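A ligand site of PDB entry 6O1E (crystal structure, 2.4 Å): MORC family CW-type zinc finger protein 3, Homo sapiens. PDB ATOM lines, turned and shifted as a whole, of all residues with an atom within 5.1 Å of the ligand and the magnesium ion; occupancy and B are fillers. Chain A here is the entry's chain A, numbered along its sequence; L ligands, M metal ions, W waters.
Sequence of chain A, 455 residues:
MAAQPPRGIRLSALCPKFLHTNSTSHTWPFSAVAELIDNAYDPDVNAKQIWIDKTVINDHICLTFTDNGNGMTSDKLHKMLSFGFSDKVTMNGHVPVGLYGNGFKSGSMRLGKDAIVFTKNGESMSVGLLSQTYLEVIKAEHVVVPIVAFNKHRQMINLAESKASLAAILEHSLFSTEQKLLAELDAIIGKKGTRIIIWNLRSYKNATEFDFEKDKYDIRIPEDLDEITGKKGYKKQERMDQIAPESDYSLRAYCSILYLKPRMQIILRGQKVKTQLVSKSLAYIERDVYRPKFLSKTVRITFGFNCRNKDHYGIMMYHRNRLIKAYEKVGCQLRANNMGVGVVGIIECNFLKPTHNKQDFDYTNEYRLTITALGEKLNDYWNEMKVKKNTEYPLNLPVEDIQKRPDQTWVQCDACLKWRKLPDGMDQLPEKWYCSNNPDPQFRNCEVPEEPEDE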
ATOM      1  N   GLU A  35      19.993 -20.792  22.062  1.00  0.00           N
ATOM      2  CA  GLU A  35      20.161 -19.491  22.710  1.00  0.00           C
ATOM      3  C   GLU A  35      21.356 -19.504  23.648  1.00  0.00           C
ATOM      4  O   GLU A  35      22.075 -18.494  23.758  1.00  0.00           O
ATOM      5  CB  GLU A  35      18.901 -19.106  23.483  1.00  0.00           C
ATOM      6  CG  GLU A  35      17.698 -18.749  22.601  1.00  0.00           C
ATOM      7  CD  GLU A  35      17.894 -17.511  21.718  1.00  0.00           C
ATOM      8  OE1 GLU A  35      18.929 -16.794  21.833  1.00  0.00           O
ATOM      9  OE2 GLU A  35      16.990 -17.261  20.883  1.00  0.00           O
ATOM     10  N   ASN A  39      25.097 -17.487  23.194  1.00  0.00           N
ATOM     11  CA  ASN A  39      25.690 -16.578  24.171  1.00  0.00           C
ATOM     12  C   ASN A  39      27.162 -16.873  24.401  1.00  0.00           C
ATOM     13  O   ASN A  39      27.974 -15.956  24.550  1.00  0.00           O
ATOM     14  CB  ASN A  39      24.907 -16.641  25.476  1.00  0.00           C
ATOM     15  CG  ASN A  39      23.560 -15.968  25.379  1.00  0.00           C
ATOM     16  OD1 ASN A  39      23.333 -15.145  24.490  1.00  0.00           O
ATOM     17  ND2 ASN A  39      22.648 -16.303  26.280  1.00  0.00           N
ATOM     18  N   ALA A  40      27.555 -18.145  24.391  1.00  0.00           N
ATOM     19  CA  ALA A  40      28.988 -18.428  24.515  1.00  0.00           C
ATOM     20  C   ALA A  40      29.729 -18.053  23.234  1.00  0.00           C
ATOM     21  O   ALA A  40      30.900 -17.658  23.282  1.00  0.00           O
ATOM     22  CB  ALA A  40      29.182 -19.900  24.864  1.00  0.00           C
ATOM     23  N   ASP A  42      29.102 -15.506  21.222  1.00  0.00           N
ATOM     24  CA  ASP A  42      29.100 -14.088  20.889  1.00  0.00           C
ATOM     25  C   ASP A  42      30.406 -13.434  21.335  1.00  0.00           C
ATOM     26  O   ASP A  42      31.075 -13.921  22.253  1.00  0.00           O
ATOM     27  CB  ASP A  42      27.899 -13.390  21.518  1.00  0.00           C
ATOM     28  CG  ASP A  42      26.716 -13.376  20.571  1.00  0.00           C
ATOM     29  OD1 ASP A  42      26.921 -13.749  19.394  1.00  0.00           O
ATOM     30  OD2 ASP A  42      25.588 -12.999  20.980  1.00  0.00           O
ATOM     31  N   ASP A  44      31.495 -10.781  22.949  1.00  0.00           N
ATOM     32  CA  ASP A  44      31.745 -10.271  24.305  1.00  0.00           C
ATOM     33  C   ASP A  44      32.101 -11.400  25.286  1.00  0.00           C
ATOM     34  O   ASP A  44      32.760 -11.142  26.299  1.00  0.00           O
ATOM     35  CB  ASP A  44      30.516  -9.497  24.821  1.00  0.00           C
ATOM     36  CG  ASP A  44      29.229 -10.336  24.766  1.00  0.00           C
ATOM     37  OD1 ASP A  44      29.089 -11.176  23.836  1.00  0.00           O
ATOM     38  OD2 ASP A  44      28.340 -10.160  25.654  1.00  0.00           O
ATOM     39  N   VAL A  45      31.635 -12.615  25.031  1.00  0.00           N
ATOM     40  CA  VAL A  45      32.041 -13.786  25.811  1.00  0.00           C
ATOM     41  C   VAL A  45      33.252 -14.463  25.189  1.00  0.00           C
ATOM     42  O   VAL A  45      34.268 -14.708  25.850  1.00  0.00           O
ATOM     43  CB  VAL A  45      30.857 -14.764  25.936  1.00  0.00           C
ATOM     44  CG1 VAL A  45      31.272 -16.041  26.667  1.00  0.00           C
ATOM     45  CG2 VAL A  45      29.717 -14.112  26.656  1.00  0.00           C
ATOM     46  N   ASP A  67      31.286 -22.942  29.633  1.00  0.00           N
ATOM     47  CA  ASP A  67      32.147 -22.354  28.627  1.00  0.00           C
ATOM     48  C   ASP A  67      33.355 -21.699  29.295  1.00  0.00           C
ATOM     49  O   ASP A  67      33.310 -21.321  30.468  1.00  0.00           O
ATOM     50  CB  ASP A  67      31.391 -21.321  27.758  1.00  0.00           C
ATOM     51  CG  ASP A  67      30.960 -20.075  28.528  1.00  0.00           C
ATOM     52  OD1 ASP A  67      29.762 -19.985  28.880  1.00  0.00           O
ATOM     53  OD2 ASP A  67      31.806 -19.178  28.773  1.00  0.00           O
ATOM     54  N   GLY A  71      33.367 -14.602  31.131  1.00  0.00           N
ATOM     55  CA  GLY A  71      32.656 -14.499  32.401  1.00  0.00           C
ATOM     56  C   GLY A  71      31.963 -13.150  32.596  1.00  0.00           C
ATOM     57  O   GLY A  71      31.883 -12.319  31.697  1.00  0.00           O
ATOM     58  N   MET A  72      31.488 -12.924  33.824  1.00  0.00           N
ATOM     59  CA  MET A  72      30.682 -11.748  34.130  1.00  0.00           C
ATOM     60  C   MET A  72      31.039 -11.160  35.484  1.00  0.00           C
ATOM     61  O   MET A  72      31.290 -11.900  36.440  1.00  0.00           O
ATOM     62  CB  MET A  72      29.188 -12.078  34.142  1.00  0.00           C
ATOM     63  CG  MET A  72      28.440 -11.835  32.850  1.00  0.00           C
ATOM     64  SD  MET A  72      26.830 -12.649  32.946  1.00  0.00           S
ATOM     65  CE  MET A  72      27.353 -14.362  33.076  1.00  0.00           C
ATOM     66  N   LYS A  76      26.877  -7.377  35.587  1.00  0.00           N
ATOM     67  CA  LYS A  76      26.369  -7.858  34.302  1.00  0.00           C
ATOM     68  C   LYS A  76      25.556  -9.130  34.473  1.00  0.00           C
ATOM     69  O   LYS A  76      24.594  -9.346  33.724  1.00  0.00           O
ATOM     70  CB  LYS A  76      27.525  -8.051  33.308  1.00  0.00           C
ATOM     71  CG  LYS A  76      28.094  -6.713  32.856  1.00  0.00           C
ATOM     72  CD  LYS A  76      27.949  -6.459  31.349  1.00  0.00           C
ATOM     73  CE  LYS A  76      28.487  -7.614  30.505  1.00  0.00           C
ATOM     74  NZ  LYS A  76      28.935  -7.137  29.160  1.00  0.00           N
ATOM     75  N   LYS A  79      22.230  -8.127  35.032  1.00  0.00           N
ATOM     76  CA  LYS A  79      21.640  -7.700  33.773  1.00  0.00           C
ATOM     77  C   LYS A  79      21.250  -8.910  32.921  1.00  0.00           C
ATOM     78  O   LYS A  79      20.175  -8.918  32.306  1.00  0.00           O
ATOM     79  CB  LYS A  79      22.615  -6.783  33.035  1.00  0.00           C
ATOM     80  CG  LYS A  79      22.252  -5.323  33.144  1.00  0.00           C
ATOM     81  CD  LYS A  79      23.484  -4.413  33.224  1.00  0.00           C
ATOM     82  CE  LYS A  79      23.036  -2.951  33.349  1.00  0.00           C
ATOM     83  NZ  LYS A  79      24.020  -2.074  34.045  1.00  0.00           N
ATOM     84  N   MET A  80      22.077  -9.952  32.931  1.00  0.00           N
ATOM     85  CA  MET A  80      21.718 -11.192  32.232  1.00  0.00           C
ATOM     86  C   MET A  80      20.459 -11.822  32.823  1.00  0.00           C
ATOM     87  O   MET A  80      19.640 -12.391  32.086  1.00  0.00           O
ATOM     88  CB  MET A  80      22.875 -12.174  32.296  1.00  0.00           C
ATOM     89  CG  MET A  80      22.495 -13.624  32.050  1.00  0.00           C
ATOM     90  SD  MET A  80      23.977 -14.638  32.165  1.00  0.00           S
ATOM     91  CE  MET A  80      23.335 -16.308  31.965  1.00  0.00           C
ATOM     92  N   PHE A  85      18.396  -6.068  28.552  1.00  0.00           N
ATOM     93  CA  PHE A  85      19.736  -5.510  28.632  1.00  0.00           C
ATOM     94  C   PHE A  85      20.620  -6.263  27.653  1.00  0.00           C
ATOM     95  O   PHE A  85      20.967  -7.431  27.892  1.00  0.00           O
ATOM     96  CB  PHE A  85      20.301  -5.585  30.050  1.00  0.00           C
ATOM     97  CG  PHE A  85      19.541  -4.765  31.035  1.00  0.00           C
ATOM     98  CD1 PHE A  85      18.430  -5.281  31.680  1.00  0.00           C
ATOM     99  CD2 PHE A  85      19.904  -3.449  31.277  1.00  0.00           C
ATOM    100  CE1 PHE A  85      17.697  -4.504  32.556  1.00  0.00           C
ATOM    101  CE2 PHE A  85      19.191  -2.686  32.154  1.00  0.00           C
ATOM    102  CZ  PHE A  85      18.083  -3.205  32.789  1.00  0.00           C
ATOM    103  N   SER A  86      20.978  -5.606  26.559  1.00  0.00           N
ATOM    104  CA  SER A  86      21.799  -6.197  25.525  1.00  0.00           C
ATOM    105  C   SER A  86      22.579  -5.052  24.922  1.00  0.00           C
ATOM    106  O   SER A  86      21.969  -4.069  24.484  1.00  0.00           O
ATOM    107  CB  SER A  86      20.933  -6.894  24.463  1.00  0.00           C
ATOM    108  OG  SER A  86      21.706  -7.556  23.483  1.00  0.00           O
ATOM    109  N   ASP A  87      23.907  -5.148  24.936  1.00  0.00           N
ATOM    110  CA  ASP A  87      24.748  -4.122  24.304  1.00  0.00           C
ATOM    111  C   ASP A  87      25.928  -4.760  23.571  1.00  0.00           C
ATOM    112  O   ASP A  87      27.085  -4.367  23.726  1.00  0.00           O
ATOM    113  CB  ASP A  87      25.197  -3.075  25.332  1.00  0.00           C
ATOM    114  CG  ASP A  87      24.067  -2.161  25.809  1.00  0.00           C
ATOM    115  OD1 ASP A  87      23.014  -2.153  25.130  1.00  0.00           O
ATOM    116  OD2 ASP A  87      24.191  -1.484  26.868  1.00  0.00           O
ATOM    117  N   LYS A  88      25.645  -5.733  22.717  1.00  0.00           N
ATOM    118  CA  LYS A  88      26.706  -6.436  22.022  1.00  0.00           C
ATOM    119  C   LYS A  88      27.124  -5.702  20.755  1.00  0.00           C
ATOM    120  O   LYS A  88      26.278  -5.190  20.014  1.00  0.00           O
ATOM    121  CB  LYS A  88      26.265  -7.856  21.680  1.00  0.00           C
ATOM    122  CG  LYS A  88      26.233  -8.784  22.885  1.00  0.00           C
ATOM    123  CD  LYS A  88      25.647 -10.132  22.537  1.00  0.00           C
ATOM    124  CE  LYS A  88      25.501 -10.973  23.786  1.00  0.00           C
ATOM    125  NZ  LYS A  88      24.827 -12.287  23.519  1.00  0.00           N
ATOM    126  N   VAL A  97      25.364 -12.421  17.409  1.00  0.00           N
ATOM    127  CA  VAL A  97      24.024 -12.816  16.973  1.00  0.00           C
ATOM    128  C   VAL A  97      22.957 -12.328  17.951  1.00  0.00           C
ATOM    129  O   VAL A  97      21.812 -12.079  17.546  1.00  0.00           O
ATOM    130  CB  VAL A  97      23.984 -14.333  16.741  1.00  0.00           C
ATOM    131  CG1 VAL A  97      25.218 -14.754  15.972  1.00  0.00           C
ATOM    132  CG2 VAL A  97      23.942 -15.106  18.045  1.00  0.00           C
ATOM    133  N   GLY A  98      23.313 -12.105  19.219  1.00  0.00           N
ATOM    134  CA  GLY A  98      22.343 -11.602  20.179  1.00  0.00           C
ATOM    135  C   GLY A  98      22.127 -10.105  20.069  1.00  0.00           C
ATOM    136  O   GLY A  98      23.011  -9.352  19.679  1.00  0.00           O
ATOM    137  N   LEU A  99      20.902  -9.677  20.384  1.00  0.00           N
ATOM    138  CA  LEU A  99      20.555  -8.268  20.329  1.00  0.00           C
ATOM    139  C   LEU A  99      19.289  -7.892  21.091  1.00  0.00           C
ATOM    140  O   LEU A  99      19.063  -6.705  21.350  1.00  0.00           O
ATOM    141  CB  LEU A  99      20.431  -7.803  18.877  1.00  0.00           C
ATOM    142  CG  LEU A  99      19.229  -8.200  18.011  1.00  0.00           C
ATOM    143  CD1 LEU A  99      18.959  -7.106  16.971  1.00  0.00           C
ATOM    144  CD2 LEU A  99      19.453  -9.568  17.326  1.00  0.00           C
ATOM    145  N   TYR A 100      18.459  -8.862  21.485  1.00  0.00           N
ATOM    146  CA  TYR A 100      17.187  -8.532  22.140  1.00  0.00           C
ATOM    147  C   TYR A 100      17.245  -8.553  23.660  1.00  0.00           C
ATOM    148  O   TYR A 100      16.314  -8.045  24.299  1.00  0.00           O
ATOM    149  CB  TYR A 100      16.097  -9.500  21.684  1.00  0.00           C
ATOM    150  CG  TYR A 100      15.722  -9.288  20.249  1.00  0.00           C
ATOM    151  CD1 TYR A 100      15.010  -8.155  19.847  1.00  0.00           C
ATOM    152  CD2 TYR A 100      16.108 -10.206  19.274  1.00  0.00           C
ATOM    153  CE1 TYR A 100      14.662  -7.952  18.512  1.00  0.00           C
ATOM    154  CE2 TYR A 100      15.776 -10.009  17.935  1.00  0.00           C
ATOM    155  CZ  TYR A 100      15.057  -8.891  17.558  1.00  0.00           C
ATOM    156  OH  TYR A 100      14.731  -8.707  16.237  1.00  0.00           O
ATOM    157  N   GLY A 101      18.289  -9.136  24.258  1.00  0.00           N
ATOM    158  CA  GLY A 101      18.354  -9.237  25.709  1.00  0.00           C
ATOM    159  C   GLY A 101      17.324 -10.171  26.324  1.00  0.00           C
ATOM    160  O   GLY A 101      16.850  -9.919  27.433  1.00  0.00           O
ATOM    161  N   ASN A 102      16.954 -11.251  25.634  1.00  0.00           N
ATOM    162  CA  ASN A 102      15.949 -12.182  26.134  1.00  0.00           C
ATOM    163  C   ASN A 102      16.356 -13.637  26.015  1.00  0.00           C
ATOM    164  O   ASN A 102      15.762 -14.476  26.696  1.00  0.00           O
ATOM    165  CB  ASN A 102      14.619 -11.981  25.408  1.00  0.00           C
ATOM    166  CG  ASN A 102      13.445 -12.524  26.207  1.00  0.00           C
ATOM    167  OD1 ASN A 102      13.484 -12.529  27.439  1.00  0.00           O
ATOM    168  ND2 ASN A 102      12.403 -12.954  25.504  1.00  0.00           N
ATOM    169  N   GLY A 103      17.390 -13.950  25.244  1.00  0.00           N
ATOM    170  CA  GLY A 103      17.679 -15.331  24.906  1.00  0.00           C
ATOM    171  C   GLY A 103      17.917 -16.222  26.109  1.00  0.00           C
ATOM    172  O   GLY A 103      17.506 -17.389  26.111  1.00  0.00           O
ATOM    173  N   PHE A 104      18.563 -15.703  27.139  1.00  0.00           N
ATOM    174  CA  PHE A 104      18.833 -16.593  28.264  1.00  0.00           C
ATOM    175  C   PHE A 104      17.590 -16.842  29.105  1.00  0.00           C
ATOM    176  O   PHE A 104      17.376 -17.971  29.567  1.00  0.00           O
ATOM    177  CB  PHE A 104      19.951 -16.055  29.153  1.00  0.00           C
ATOM    178  CG  PHE A 104      20.152 -16.885  30.368  1.00  0.00           C
ATOM    179  CD1 PHE A 104      20.798 -18.116  30.284  1.00  0.00           C
ATOM    180  CD2 PHE A 104      19.619 -16.496  31.588  1.00  0.00           C
ATOM    181  CE1 PHE A 104      20.939 -18.898  31.385  1.00  0.00           C
ATOM    182  CE2 PHE A 104      19.765 -17.287  32.693  1.00  0.00           C
ATOM    183  CZ  PHE A 104      20.419 -18.486  32.590  1.00  0.00           C
ATOM    184  N   LYS A 105      16.771 -15.811  29.357  1.00  0.00           N
ATOM    185  CA  LYS A 105      15.551 -15.988  30.147  1.00  0.00           C
ATOM    186  C   LYS A 105      14.560 -16.890  29.435  1.00  0.00           C
ATOM    187  O   LYS A 105      13.986 -17.808  30.039  1.00  0.00           O
ATOM    188  CB  LYS A 105      14.892 -14.638  30.430  1.00  0.00           C
ATOM    189  CG  LYS A 105      15.541 -13.817  31.545  1.00  0.00           C
ATOM    190  CD  LYS A 105      16.894 -13.288  31.119  1.00  0.00           C
ATOM    191  CE  LYS A 105      16.800 -12.465  29.831  1.00  0.00           C
ATOM    192  NZ  LYS A 105      18.118 -11.819  29.598  1.00  0.00           N
ATOM    193  N   THR A 194      32.114 -19.618  32.701  1.00  0.00           N
ATOM    194  CA  THR A 194      30.784 -19.618  33.295  1.00  0.00           C
ATOM    195  C   THR A 194      30.115 -20.979  33.101  1.00  0.00           C
ATOM    196  O   THR A 194      30.448 -21.739  32.199  1.00  0.00           O
ATOM    197  CB  THR A 194      29.920 -18.468  32.738  1.00  0.00           C
ATOM    198  OG1 THR A 194      28.547 -18.680  33.081  1.00  0.00           O
ATOM    199  CG2 THR A 194      30.080 -18.307  31.252  1.00  0.00           C
ATOM    200  N   ILE A 196      26.236 -23.003  33.679  1.00  0.00           N
ATOM    201  CA  ILE A 196      24.798 -22.870  33.893  1.00  0.00           C
ATOM    202  C   ILE A 196      24.256 -24.267  34.130  1.00  0.00           C
ATOM    203  O   ILE A 196      24.593 -25.217  33.405  1.00  0.00           O
ATOM    204  CB  ILE A 196      24.100 -22.209  32.696  1.00  0.00           C
ATOM    205  CG1 ILE A 196      24.757 -20.886  32.345  1.00  0.00           C
ATOM    206  CG2 ILE A 196      22.603 -22.004  32.965  1.00  0.00           C
ATOM    207  CD1 ILE A 196      24.526 -20.471  30.875  1.00  0.00           C
ATOM    208  N   LYS A 358      15.028 -16.724  16.059  1.00  0.00           N
ATOM    209  CA  LYS A 358      16.026 -17.038  15.032  1.00  0.00           C
ATOM    210  C   LYS A 358      15.832 -18.434  14.464  1.00  0.00           C
ATOM    211  O   LYS A 358      16.791 -19.190  14.252  1.00  0.00           O
ATOM    212  CB  LYS A 358      17.449 -16.831  15.571  1.00  0.00           C
ATOM    213  CG  LYS A 358      17.721 -15.364  16.030  1.00  0.00           C
ATOM    214  CD  LYS A 358      18.998 -15.218  16.885  1.00  0.00           C
ATOM    215  CE  LYS A 358      19.066 -13.825  17.546  1.00  0.00           C
ATOM    216  NZ  LYS A 358      18.583 -13.777  18.988  1.00  0.00           N
HETATM  217  P1  LIG L   1      19.338 -12.163  22.566  1.00  0.00           P
HETATM  218  O1  LIG L   1      20.001 -13.503  22.734  1.00  0.00           O
HETATM  219  O2  LIG L   1      18.067 -12.077  23.393  1.00  0.00           O
HETATM  220  O3  LIG L   1      19.049 -12.030  21.085  1.00  0.00           O
HETATM  221  P2  LIG L   1      21.420 -11.109  24.379  1.00  0.00           P
HETATM  222  O4  LIG L   1      22.336 -12.273  24.061  1.00  0.00           O
HETATM  223  O5  LIG L   1      22.193  -9.853  24.676  1.00  0.00           O
HETATM  224  N1  LIG L   1      20.355 -10.878  23.087  1.00  0.00           N
HETATM  225  P3  LIG L   1      20.627 -12.857  26.569  1.00  0.00           P
HETATM  226  O6  LIG L   1      20.862 -14.115  25.751  1.00  0.00           O
HETATM  227  O7  LIG L   1      19.431 -12.942  27.491  1.00  0.00           O
HETATM  228  O8  LIG L   1      20.433 -11.496  25.639  1.00  0.00           O
HETATM  229  O9  LIG L   1      21.985 -12.563  27.489  1.00  0.00           O
HETATM  230  C1  LIG L   1      21.898 -11.387  28.240  1.00  0.00           C
HETATM  231  C2  LIG L   1      23.359 -10.986  28.614  1.00  0.00           C
HETATM  232  O10 LIG L   1      23.879 -11.890  29.394  1.00  0.00           O
HETATM  233  C3  LIG L   1      24.175 -11.044  27.329  1.00  0.00           C
HETATM  234  O11 LIG L   1      24.078  -9.826  26.723  1.00  0.00           O
HETATM  235  C4  LIG L   1      25.596 -11.381  27.866  1.00  0.00           C
HETATM  236  O12 LIG L   1      26.296 -10.076  28.067  1.00  0.00           O
HETATM  237  C5  LIG L   1      25.433 -12.026  29.009  1.00  0.00           C
HETATM  238  N2  LIG L   1      25.691 -13.465  28.902  1.00  0.00           N
HETATM  239  C6  LIG L   1      24.809 -14.415  28.541  1.00  0.00           C
HETATM  240  N3  LIG L   1      25.423 -15.616  28.569  1.00  0.00           N
HETATM  241  C7  LIG L   1      26.702 -15.390  28.976  1.00  0.00           C
HETATM  242  C8  LIG L   1      27.767 -16.245  29.187  1.00  0.00           C
HETATM  243  N4  LIG L   1      27.900 -17.676  29.026  1.00  0.00           N
HETATM  244  N5  LIG L   1      28.946 -15.782  29.580  1.00  0.00           N
HETATM  245  C9  LIG L   1      29.102 -14.444  29.802  1.00  0.00           C
HETATM  246  N6  LIG L   1      28.066 -13.598  29.592  1.00  0.00           N
HETATM  247  C10 LIG L   1      26.868 -14.067  29.184  1.00  0.00           C
HETATM  248 MG    MG M   1      21.556 -14.232  23.793  1.00  0.00          MG
HETATM  249  O   HOH W   1      22.498 -14.263  21.953  1.00  0.00           O
HETATM  250  O   HOH W   2      25.082  -7.428  26.470  1.00  0.00           O
HETATM  251  O   HOH W   3      27.826  -7.685  26.649  1.00  0.00           O
HETATM  252  O   HOH W   4      23.649 -17.828  28.406  1.00  0.00           O
HETATM  253  O   HOH W   5      20.875 -16.193  23.569  1.00  0.00           O
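The side-chain sulfur (SD) of Met 72 lies close to a nitrogen (N6) of the ligand, at 3.7 Å. Glu 35 touches the ligand. Val 45 touches the ligand. O of Gly 71 touches C9 of the ligand (3.98 Å). Met 80 touches the ligand. Gly 98 touches the ligand. CG2 of Thr 194 touches N4 of the ligand (3.2 Å). Within 4 Å of the ligand: Glu 35, Asn 39, Asp 44, Val 45, Asp 67, Gly 71, Met 72, Met 80, Ser 86, Lys 88, Gly 98, Leu 99, Tyr 100, Gly 101, Asn 102, Gly 103, Phe 104, Lys 105, Thr 194 and Lys 358. The nearest printed residue that does not touch the ligand is Phe 85 (4.1 Å).
The magnesium ion is bound by O1 of the ligand (2.0 Å), water W1 (2.1 Å), O6 of the ligand (2.1 Å), water W5 (2.1 Å), OD1 of Asn 39 (2.1 Å) and O4 of the ligand (2.1 Å). The magnesium ion has six donor atoms within binding distance.
Lys 88 touches the magnesium ion. Within 4 Å of the magnesium ion: Asn 39 and Lys 88. The nearest printed residue that does not touch the magnesium ion is Glu 35 (4.2 Å).
NZ of Lys 358 lies within salt-bridge range of O3 of the ligand. O2 of the ligand sits at hydrogen-bond distance from N of Gly 101 (3.1 Å). The side-chain carboxylate (OD1) of Asp 67 is in hydrogen-bond range of a nitrogen (N4) of the ligand, at 3.0 Å. N of Asn 102 lies within hydrogen-bond range of O2 of the ligand (2.6 Å). O2 of the ligand is in hydrogen-bond range of N of Gly 103, at 2.7 Å. N of Tyr 100 sits at hydrogen-bond distance from O3 of the ligand. The side-chain hydroxyl (OG) of Ser 86 is in hydrogen-bond range of an oxygen (O5) of the ligand, 2.6 Å away. The backbone NH of Phe 104 lies within hydrogen-bond range of an oxygen (O7) of the ligand, 2.9 Å away. NZ of Lys 88 lies within salt-bridge range of O5 of the ligand. An oxygen (O7) of the ligand is in salt-bridge range of the side-chain amino group (NZ) of Lys 105 (2.7 Å). An oxygen (O3) of the ligand lies within hydrogen-bond range of the backbone NH (N) of Leu 99 (3.1 Å). The side-chain carboxylate (OD2) of Asp 44 lies within hydrogen-bond range of an oxygen (O12) of the ligand (3.2 Å).
Water W1 bridges NZ of Lys 88 (3.4 Å) and OD2 of Asp 42 (3.5 Å). Water W5 lies within hydrogen-bond range of O of Glu 35 and ND2 of Asn 39. Water W2 lies within hydrogen-bond range of O11 of the ligand (2.6 Å) and N of Asp 87 (3.0 Å). Water W4 bridges the side-chain amide nitrogen of Asn 39 and a nitrogen (N3) of the ligand. Water W3 lies within hydrogen-bond range of the side-chain carboxylate (OD2) of Asp 44 (2.7 Å), the side-chain amino group (NZ) of Lys 76 (2.8 Å) and an oxygen (O12) of the ligand (3.2 Å).
The backbone carbonyl oxygen of Gly 101 is in hydrogen-bond range of the side-chain amino group of Lys 105 (3.1 Å). The side-chain amino group (NZ) of Lys 88 is in salt-bridge range of the side-chain carboxylate (OD2) of Asp 42, 2.7 Å away. N of Gly 98 lies within hydrogen-bond range of OD2 of Asp 42 (3.0 Å). The backbone carbonyl oxygen (O) of Glu 35 lies close to the side-chain amide nitrogen (ND2) of Asn 39 (3.4 Å). The side-chain amide oxygen (OD1) of Asn 39 lies close to the side-chain amino group (NZ) of Lys 88 (3.4 Å). O of Thr 194 is in hydrogen-bond range of N of Asp 67 (3.0 Å). The side-chain amino group (NZ) of Lys 105 lies within hydrogen-bond range of the backbone carbonyl oxygen (O) of Met 80 (3.0 Å).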
